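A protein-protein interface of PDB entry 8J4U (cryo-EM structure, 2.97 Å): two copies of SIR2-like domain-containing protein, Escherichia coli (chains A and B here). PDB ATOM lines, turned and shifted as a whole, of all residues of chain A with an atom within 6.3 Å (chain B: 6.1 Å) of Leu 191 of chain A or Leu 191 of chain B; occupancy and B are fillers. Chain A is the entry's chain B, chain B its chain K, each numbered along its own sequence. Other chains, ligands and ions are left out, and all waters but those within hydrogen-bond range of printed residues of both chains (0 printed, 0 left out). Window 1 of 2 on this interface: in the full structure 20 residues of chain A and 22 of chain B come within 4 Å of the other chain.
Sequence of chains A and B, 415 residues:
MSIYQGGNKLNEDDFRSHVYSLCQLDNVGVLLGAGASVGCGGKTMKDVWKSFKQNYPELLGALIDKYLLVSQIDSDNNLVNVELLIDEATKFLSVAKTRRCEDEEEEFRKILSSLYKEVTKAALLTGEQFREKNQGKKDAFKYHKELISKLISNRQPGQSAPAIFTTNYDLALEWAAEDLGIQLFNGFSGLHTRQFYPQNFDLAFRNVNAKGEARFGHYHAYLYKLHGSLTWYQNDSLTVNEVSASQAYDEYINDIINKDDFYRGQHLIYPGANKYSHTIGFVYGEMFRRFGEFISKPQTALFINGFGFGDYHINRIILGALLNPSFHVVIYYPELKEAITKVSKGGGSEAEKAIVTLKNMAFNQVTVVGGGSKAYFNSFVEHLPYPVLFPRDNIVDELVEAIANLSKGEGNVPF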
ATOM      1  N   GLU A 178     -15.987   0.013  16.203  1.00  0.00           N
ATOM      2  CA  GLU A 178     -16.422  -0.501  17.494  1.00  0.00           C
ATOM      3  C   GLU A 178     -17.616  -1.435  17.366  1.00  0.00           C
ATOM      4  O   GLU A 178     -17.960  -2.110  18.342  1.00  0.00           O
ATOM      5  CB  GLU A 178     -16.764   0.656  18.431  1.00  0.00           C
ATOM      6  CG  GLU A 178     -15.574   1.185  19.210  1.00  0.00           C
ATOM      7  CD  GLU A 178     -15.814   2.563  19.779  1.00  0.00           C
ATOM      8  OE1 GLU A 178     -14.829   3.225  20.167  1.00  0.00           O
ATOM      9  OE2 GLU A 178     -16.985   2.987  19.840  1.00  0.00           O
ATOM     10  N   SER A 189      -3.110   5.711  24.712  1.00  0.00           N
ATOM     11  CA  SER A 189      -3.106   4.553  25.595  1.00  0.00           C
ATOM     12  C   SER A 189      -3.668   4.948  26.952  1.00  0.00           C
ATOM     13  O   SER A 189      -3.415   6.054  27.434  1.00  0.00           O
ATOM     14  CB  SER A 189      -1.693   3.990  25.755  1.00  0.00           C
ATOM     15  OG  SER A 189      -1.687   2.855  26.599  1.00  0.00           O
ATOM     16  N   GLY A 190      -4.422   4.042  27.558  1.00  0.00           N
ATOM     17  CA  GLY A 190      -4.984   4.229  28.880  1.00  0.00           C
ATOM     18  C   GLY A 190      -6.476   4.509  28.835  1.00  0.00           C
ATOM     19  O   GLY A 190      -7.059   4.806  27.792  1.00  0.00           O
ATOM     20  N   LEU A 191      -7.098   4.397  30.008  1.00  0.00           N
ATOM     21  CA  LEU A 191      -8.518   4.685  30.158  1.00  0.00           C
ATOM     22  C   LEU A 191      -8.797   5.827  31.121  1.00  0.00           C
ATOM     23  O   LEU A 191      -9.489   6.782  30.753  1.00  0.00           O
ATOM     24  CB  LEU A 191      -9.266   3.426  30.617  1.00  0.00           C
ATOM     25  CG  LEU A 191     -10.767   3.618  30.834  1.00  0.00           C
ATOM     26  CD1 LEU A 191     -11.461   3.893  29.530  1.00  0.00           C
ATOM     27  CD2 LEU A 191     -11.363   2.410  31.497  1.00  0.00           C
ATOM     28  N   HIS A 192      -8.284   5.757  32.349  1.00  0.00           N
ATOM     29  CA  HIS A 192      -8.569   6.801  33.325  1.00  0.00           C
ATOM     30  C   HIS A 192      -7.708   8.034  33.098  1.00  0.00           C
ATOM     31  O   HIS A 192      -8.123   9.147  33.438  1.00  0.00           O
ATOM     32  CB  HIS A 192      -8.358   6.270  34.742  1.00  0.00           C
ATOM     33  CG  HIS A 192      -9.093   5.000  35.032  1.00  0.00           C
ATOM     34  ND1 HIS A 192     -10.461   4.885  34.905  1.00  0.00           N
ATOM     35  CD2 HIS A 192      -8.653   3.791  35.452  1.00  0.00           C
ATOM     36  CE1 HIS A 192     -10.828   3.657  35.226  1.00  0.00           C
ATOM     37  NE2 HIS A 192      -9.751   2.974  35.563  1.00  0.00           N
ATOM     38  N   THR A 193      -6.515   7.856  32.539  1.00  0.00           N
ATOM     39  CA  THR A 193      -5.670   8.964  32.110  1.00  0.00           C
ATOM     40  C   THR A 193      -5.020   8.540  30.802  1.00  0.00           C
ATOM     41  O   THR A 193      -4.111   7.705  30.802  1.00  0.00           O
ATOM     42  CB  THR A 193      -4.622   9.308  33.166  1.00  0.00           C
ATOM     43  OG1 THR A 193      -5.272   9.586  34.411  1.00  0.00           O
ATOM     44  CG2 THR A 193      -3.824  10.522  32.759  1.00  0.00           C
ATOM     45  N   ARG A 194      -5.483   9.109  29.694  1.00  0.00           N
ATOM     46  CA  ARG A 194      -5.062   8.709  28.359  1.00  0.00           C
ATOM     47  C   ARG A 194      -4.036   9.701  27.832  1.00  0.00           C
ATOM     48  O   ARG A 194      -4.232  10.916  27.935  1.00  0.00           O
ATOM     49  CB  ARG A 194      -6.268   8.626  27.425  1.00  0.00           C
ATOM     50  CG  ARG A 194      -6.216   7.485  26.432  1.00  0.00           C
ATOM     51  CD  ARG A 194      -7.578   7.187  25.853  1.00  0.00           C
ATOM     52  NE  ARG A 194      -7.496   6.531  24.553  1.00  0.00           N
ATOM     53  CZ  ARG A 194      -7.405   5.219  24.377  1.00  0.00           C
ATOM     54  NH1 ARG A 194      -7.376   4.397  25.412  1.00  0.00           N
ATOM     55  NH2 ARG A 194      -7.335   4.724  23.156  1.00  0.00           N
ATOM     56  N   GLU A 242      -6.834  12.440  25.632  1.00  0.00           N
ATOM     57  CA  GLU A 242      -8.005  11.996  24.894  1.00  0.00           C
ATOM     58  C   GLU A 242      -9.123  11.634  25.860  1.00  0.00           C
ATOM     59  O   GLU A 242      -8.883  11.222  26.997  1.00  0.00           O
ATOM     60  CB  GLU A 242      -7.678  10.792  24.014  1.00  0.00           C
ATOM     61  CG  GLU A 242      -8.800  10.381  23.082  1.00  0.00           C
ATOM     62  CD  GLU A 242      -8.456   9.177  22.229  1.00  0.00           C
ATOM     63  OE1 GLU A 242      -7.773   8.262  22.733  1.00  0.00           O
ATOM     64  OE2 GLU A 242      -8.877   9.138  21.055  1.00  0.00           O
ATOM     65  N   VAL A 243     -10.359  11.793  25.390  1.00  0.00           N
ATOM     66  CA  VAL A 243     -11.541  11.556  26.210  1.00  0.00           C
ATOM     67  C   VAL A 243     -12.653  11.019  25.322  1.00  0.00           C
ATOM     68  O   VAL A 243     -12.615  11.148  24.099  1.00  0.00           O
ATOM     69  CB  VAL A 243     -11.960  12.852  26.946  1.00  0.00           C
ATOM     70  CG1 VAL A 243     -13.293  12.710  27.584  1.00  0.00           C
ATOM     71  CG2 VAL A 243     -10.941  13.178  28.000  1.00  0.00           C
ATOM     72  N   SER A 244     -13.643  10.389  25.945  1.00  0.00           N
ATOM     73  CA  SER A 244     -14.767   9.827  25.212  1.00  0.00           C
ATOM     74  C   SER A 244     -15.695  10.954  24.770  1.00  0.00           C
ATOM     75  O   SER A 244     -15.394  12.140  24.926  1.00  0.00           O
ATOM     76  CB  SER A 244     -15.491   8.791  26.064  1.00  0.00           C
ATOM     77  OG  SER A 244     -16.215   9.407  27.108  1.00  0.00           O
ATOM     78  N   ALA A 245     -16.849  10.591  24.219  1.00  0.00           N
ATOM     79  CA  ALA A 245     -17.745  11.544  23.584  1.00  0.00           C
ATOM     80  C   ALA A 245     -18.873  12.010  24.491  1.00  0.00           C
ATOM     81  O   ALA A 245     -19.720  12.788  24.047  1.00  0.00           O
ATOM     82  CB  ALA A 245     -18.330  10.939  22.310  1.00  0.00           C
ATOM     83  N   GLN A 247     -18.070  12.669  28.252  1.00  0.00           N
ATOM     84  CA  GLN A 247     -17.319  13.616  29.066  1.00  0.00           C
ATOM     85  C   GLN A 247     -17.189  14.960  28.360  1.00  0.00           C
ATOM     86  O   GLN A 247     -17.381  16.021  28.966  1.00  0.00           O
ATOM     87  CB  GLN A 247     -15.936  13.046  29.365  1.00  0.00           C
ATOM     88  CG  GLN A 247     -15.847  12.092  30.529  1.00  0.00           C
ATOM     89  CD  GLN A 247     -14.410  11.819  30.921  1.00  0.00           C
ATOM     90  OE1 GLN A 247     -13.493  12.505  30.473  1.00  0.00           O
ATOM     91  NE2 GLN A 247     -14.202  10.807  31.746  1.00  0.00           N
ATOM     92  N   GLU B 174      -4.504  -0.413  38.550  1.00  0.00           N
ATOM     93  CA  GLU B 174      -4.681   0.348  37.320  1.00  0.00           C
ATOM     94  C   GLU B 174      -4.092   1.747  37.452  1.00  0.00           C
ATOM     95  O   GLU B 174      -3.376   2.218  36.561  1.00  0.00           O
ATOM     96  CB  GLU B 174      -6.164   0.422  36.967  1.00  0.00           C
ATOM     97  CG  GLU B 174      -6.897  -0.898  37.112  1.00  0.00           C
ATOM     98  CD  GLU B 174      -8.241  -0.900  36.416  1.00  0.00           C
ATOM     99  OE1 GLU B 174      -8.735   0.192  36.067  1.00  0.00           O
ATOM    100  OE2 GLU B 174      -8.805  -1.995  36.214  1.00  0.00           O
ATOM    101  N   GLU B 178      -0.996   2.825  34.967  1.00  0.00           N
ATOM    102  CA  GLU B 178      -1.175   3.995  34.118  1.00  0.00           C
ATOM    103  C   GLU B 178      -0.083   5.032  34.325  1.00  0.00           C
ATOM    104  O   GLU B 178       0.169   5.838  33.424  1.00  0.00           O
ATOM    105  CB  GLU B 178      -2.534   4.637  34.382  1.00  0.00           C
ATOM    106  CG  GLU B 178      -3.644   4.154  33.477  1.00  0.00           C
ATOM    107  CD  GLU B 178      -4.986   4.728  33.859  1.00  0.00           C
ATOM    108  OE1 GLU B 178      -5.023   5.609  34.742  1.00  0.00           O
ATOM    109  OE2 GLU B 178      -6.006   4.299  33.282  1.00  0.00           O
ATOM    110  N   SER B 189     -12.452  -3.880  25.482  1.00  0.00           N
ATOM    111  CA  SER B 189     -11.938  -3.286  24.248  1.00  0.00           C
ATOM    112  C   SER B 189     -12.881  -2.187  23.787  1.00  0.00           C
ATOM    113  O   SER B 189     -14.084  -2.426  23.647  1.00  0.00           O
ATOM    114  CB  SER B 189     -11.788  -4.349  23.167  1.00  0.00           C
ATOM    115  OG  SER B 189     -11.020  -5.444  23.629  1.00  0.00           O
ATOM    116  N   GLY B 190     -12.343  -1.001  23.543  1.00  0.00           N
ATOM    117  CA  GLY B 190     -13.111   0.138  23.081  1.00  0.00           C
ATOM    118  C   GLY B 190     -13.033   1.308  24.047  1.00  0.00           C
ATOM    119  O   GLY B 190     -12.561   1.195  25.176  1.00  0.00           O
ATOM    120  N   LEU B 191     -13.507   2.453  23.564  1.00  0.00           N
ATOM    121  CA  LEU B 191     -13.560   3.647  24.405  1.00  0.00           C
ATOM    122  C   LEU B 191     -14.927   4.312  24.436  1.00  0.00           C
ATOM    123  O   LEU B 191     -15.343   4.788  25.493  1.00  0.00           O
ATOM    124  CB  LEU B 191     -12.513   4.663  23.942  1.00  0.00           C
ATOM    125  CG  LEU B 191     -12.328   5.858  24.878  1.00  0.00           C
ATOM    126  CD1 LEU B 191     -11.535   5.462  26.112  1.00  0.00           C
ATOM    127  CD2 LEU B 191     -11.654   6.995  24.163  1.00  0.00           C
ATOM    128  N   HIS B 192     -15.636   4.362  23.310  1.00  0.00           N
ATOM    129  CA  HIS B 192     -16.971   4.947  23.314  1.00  0.00           C
ATOM    130  C   HIS B 192     -18.028   3.927  23.707  1.00  0.00           C
ATOM    131  O   HIS B 192     -19.013   4.281  24.361  1.00  0.00           O
ATOM    132  CB  HIS B 192     -17.285   5.546  21.946  1.00  0.00           C
ATOM    133  CG  HIS B 192     -16.213   6.450  21.424  1.00  0.00           C
ATOM    134  ND1 HIS B 192     -16.066   7.751  21.852  1.00  0.00           N
ATOM    135  CD2 HIS B 192     -15.236   6.243  20.511  1.00  0.00           C
ATOM    136  CE1 HIS B 192     -15.041   8.303  21.229  1.00  0.00           C
ATOM    137  NE2 HIS B 192     -14.521   7.411  20.409  1.00  0.00           N
ATOM    138  N   THR B 193     -17.842   2.669  23.315  1.00  0.00           N
ATOM    139  CA  THR B 193     -18.562   1.542  23.894  1.00  0.00           C
ATOM    140  C   THR B 193     -17.541   0.456  24.173  1.00  0.00           C
ATOM    141  O   THR B 193     -16.933  -0.078  23.242  1.00  0.00           O
ATOM    142  CB  THR B 193     -19.663   1.015  22.970  1.00  0.00           C
ATOM    143  OG1 THR B 193     -19.075   0.437  21.799  1.00  0.00           O
ATOM    144  CG2 THR B 193     -20.606   2.119  22.576  1.00  0.00           C
ATOM    145  N   ARG B 194     -17.356   0.138  25.446  1.00  0.00           N
ATOM    146  CA  ARG B 194     -16.363  -0.826  25.890  1.00  0.00           C
ATOM    147  C   ARG B 194     -17.085  -2.096  26.315  1.00  0.00           C
ATOM    148  O   ARG B 194     -18.017  -2.041  27.124  1.00  0.00           O
ATOM    149  CB  ARG B 194     -15.545  -0.234  27.037  1.00  0.00           C
ATOM    150  CG  ARG B 194     -14.238  -0.921  27.333  1.00  0.00           C
ATOM    151  CD  ARG B 194     -13.322  -0.002  28.117  1.00  0.00           C
ATOM    152  NE  ARG B 194     -12.261   0.564  27.295  1.00  0.00           N
ATOM    153  CZ  ARG B 194     -10.992   0.166  27.302  1.00  0.00           C
ATOM    154  NH1 ARG B 194     -10.587  -0.813  28.098  1.00  0.00           N
ATOM    155  NH2 ARG B 194     -10.118   0.761  26.504  1.00  0.00           N
ATOM    156  N   GLU B 242     -18.021  -1.011  30.535  1.00  0.00           N
ATOM    157  CA  GLU B 242     -17.031  -0.434  31.433  1.00  0.00           C
ATOM    158  C   GLU B 242     -16.911   1.057  31.167  1.00  0.00           C
ATOM    159  O   GLU B 242     -17.007   1.503  30.021  1.00  0.00           O
ATOM    160  CB  GLU B 242     -15.664  -1.093  31.255  1.00  0.00           C
ATOM    161  CG  GLU B 242     -14.689  -0.790  32.366  1.00  0.00           C
ATOM    162  CD  GLU B 242     -13.288  -1.293  32.083  1.00  0.00           C
ATOM    163  OE1 GLU B 242     -12.987  -1.609  30.917  1.00  0.00           O
ATOM    164  OE2 GLU B 242     -12.483  -1.376  33.033  1.00  0.00           O
ATOM    165  N   VAL B 243     -16.696   1.827  32.233  1.00  0.00           N
ATOM    166  CA  VAL B 243     -16.522   3.272  32.104  1.00  0.00           C
ATOM    167  C   VAL B 243     -15.346   3.736  32.950  1.00  0.00           C
ATOM    168  O   VAL B 243     -14.645   2.927  33.566  1.00  0.00           O
ATOM    169  CB  VAL B 243     -17.799   4.042  32.490  1.00  0.00           C
ATOM    170  CG1 VAL B 243     -18.857   3.871  31.439  1.00  0.00           C
ATOM    171  CG2 VAL B 243     -18.311   3.602  33.836  1.00  0.00           C
ATOM    172  N   SER B 244     -15.122   5.044  32.970  1.00  0.00           N
ATOM    173  CA  SER B 244     -14.060   5.675  33.735  1.00  0.00           C
ATOM    174  C   SER B 244     -14.593   6.170  35.073  1.00  0.00           C
ATOM    175  O   SER B 244     -15.802   6.285  35.285  1.00  0.00           O
ATOM    176  CB  SER B 244     -13.453   6.835  32.946  1.00  0.00           C
ATOM    177  OG  SER B 244     -12.385   7.433  33.648  1.00  0.00           O
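The side-chain carboxylate (OE1) of Glu 178 of chain A sits close to the backbone NH (N) of His 192 of chain B (3.4 Å).
The side-chain carboxylate (OE2) of Glu 178 of chain B lies within hydrogen-bond range of the backbone NH (N) of Leu 191 of chain A (3.5 Å).
NE2 of His 192 of chain A is in hydrogen-bond range of OE1 of Glu 174 of chain B.
N of His 192 of chain A is in hydrogen-bond range of OE2 of Glu 178 of chain B, 2.9 Å away.
A ring nitrogen (ND1) of His 192 of chain A is in hydrogen-bond range of the side-chain hydroxyl (OG) of Ser 244 of chain B, 3.4 Å away.
The side-chain carboxylate (OE1) of Glu 178 of chain B is in hydrogen-bond range of the backbone NH (N) of Thr 193 of chain A (3.5 Å).
Leu 191 of chain B touches Glu 178 of chain A (N to OE1, 3.7 Å).
Thr 193 of chain B touches Glu 178 of chain A.
Leu 191 of chain A touches Leu 191 of chain B (CD1 to CD1, 3.8 Å).
CD2 of Leu 191 of chain A touches O of Val 243 of chain B, at 3.9 Å.
N of Ala 245 of chain A touches ND1 of His 192 of chain B, 3.8 Å away.
Leu 191 of chain A touches three residues of chain B.
Printed residues of chain A within 4 Å of Glu 178 of chain B: Leu 191 (3.5 Å), His 192 (2.9 Å) and Thr 193 (3.5 Å).
Leu 191 of chain B touches two residues of chain A.
Of the printed residues of chain A, Thr 193 of chain B touches Glu 178.
Glu 242 of chain B touches none of the printed residues of chain A.
The nearest residue of chain A that does not touch Leu 191 of chain B is Ser 244 of chain A (4.05 Å).
Printed residues of chain A that touch a printed residue of chain B: Glu 178, Leu 191, His 192, Thr 193 and Ala 245.
Hydrophobic or aromatic side chains of chain A within 4 Å of the printed part of chain B: Leu 191, His 192 and Ala 245.
Among the printed residues, 11 pairs touch across the chains.
Glu 178 of chain A touches Leu 191 of chain B, and with the chains exchanged Leu 191 of chain A touches Glu 178 of chain B.
Leu 191 of chain A touches its own counterpart, Leu 191 of chain B.
Leu 191 of chain A touches Val 243 of chain B, but with the chains exchanged Val 243 of chain A does not touch Leu 191 of chain B (4.3 Å).
His 192 of chain A touches Ser 244 of chain B, but with the chains exchanged Ser 244 of chain A does not touch His 192 of chain B (4.2 Å).
10 positions are printed for both chains.
Of the 11 pairs that touch across the chains among the printed residues, 7 have their exchanged pair printed and touching as well.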
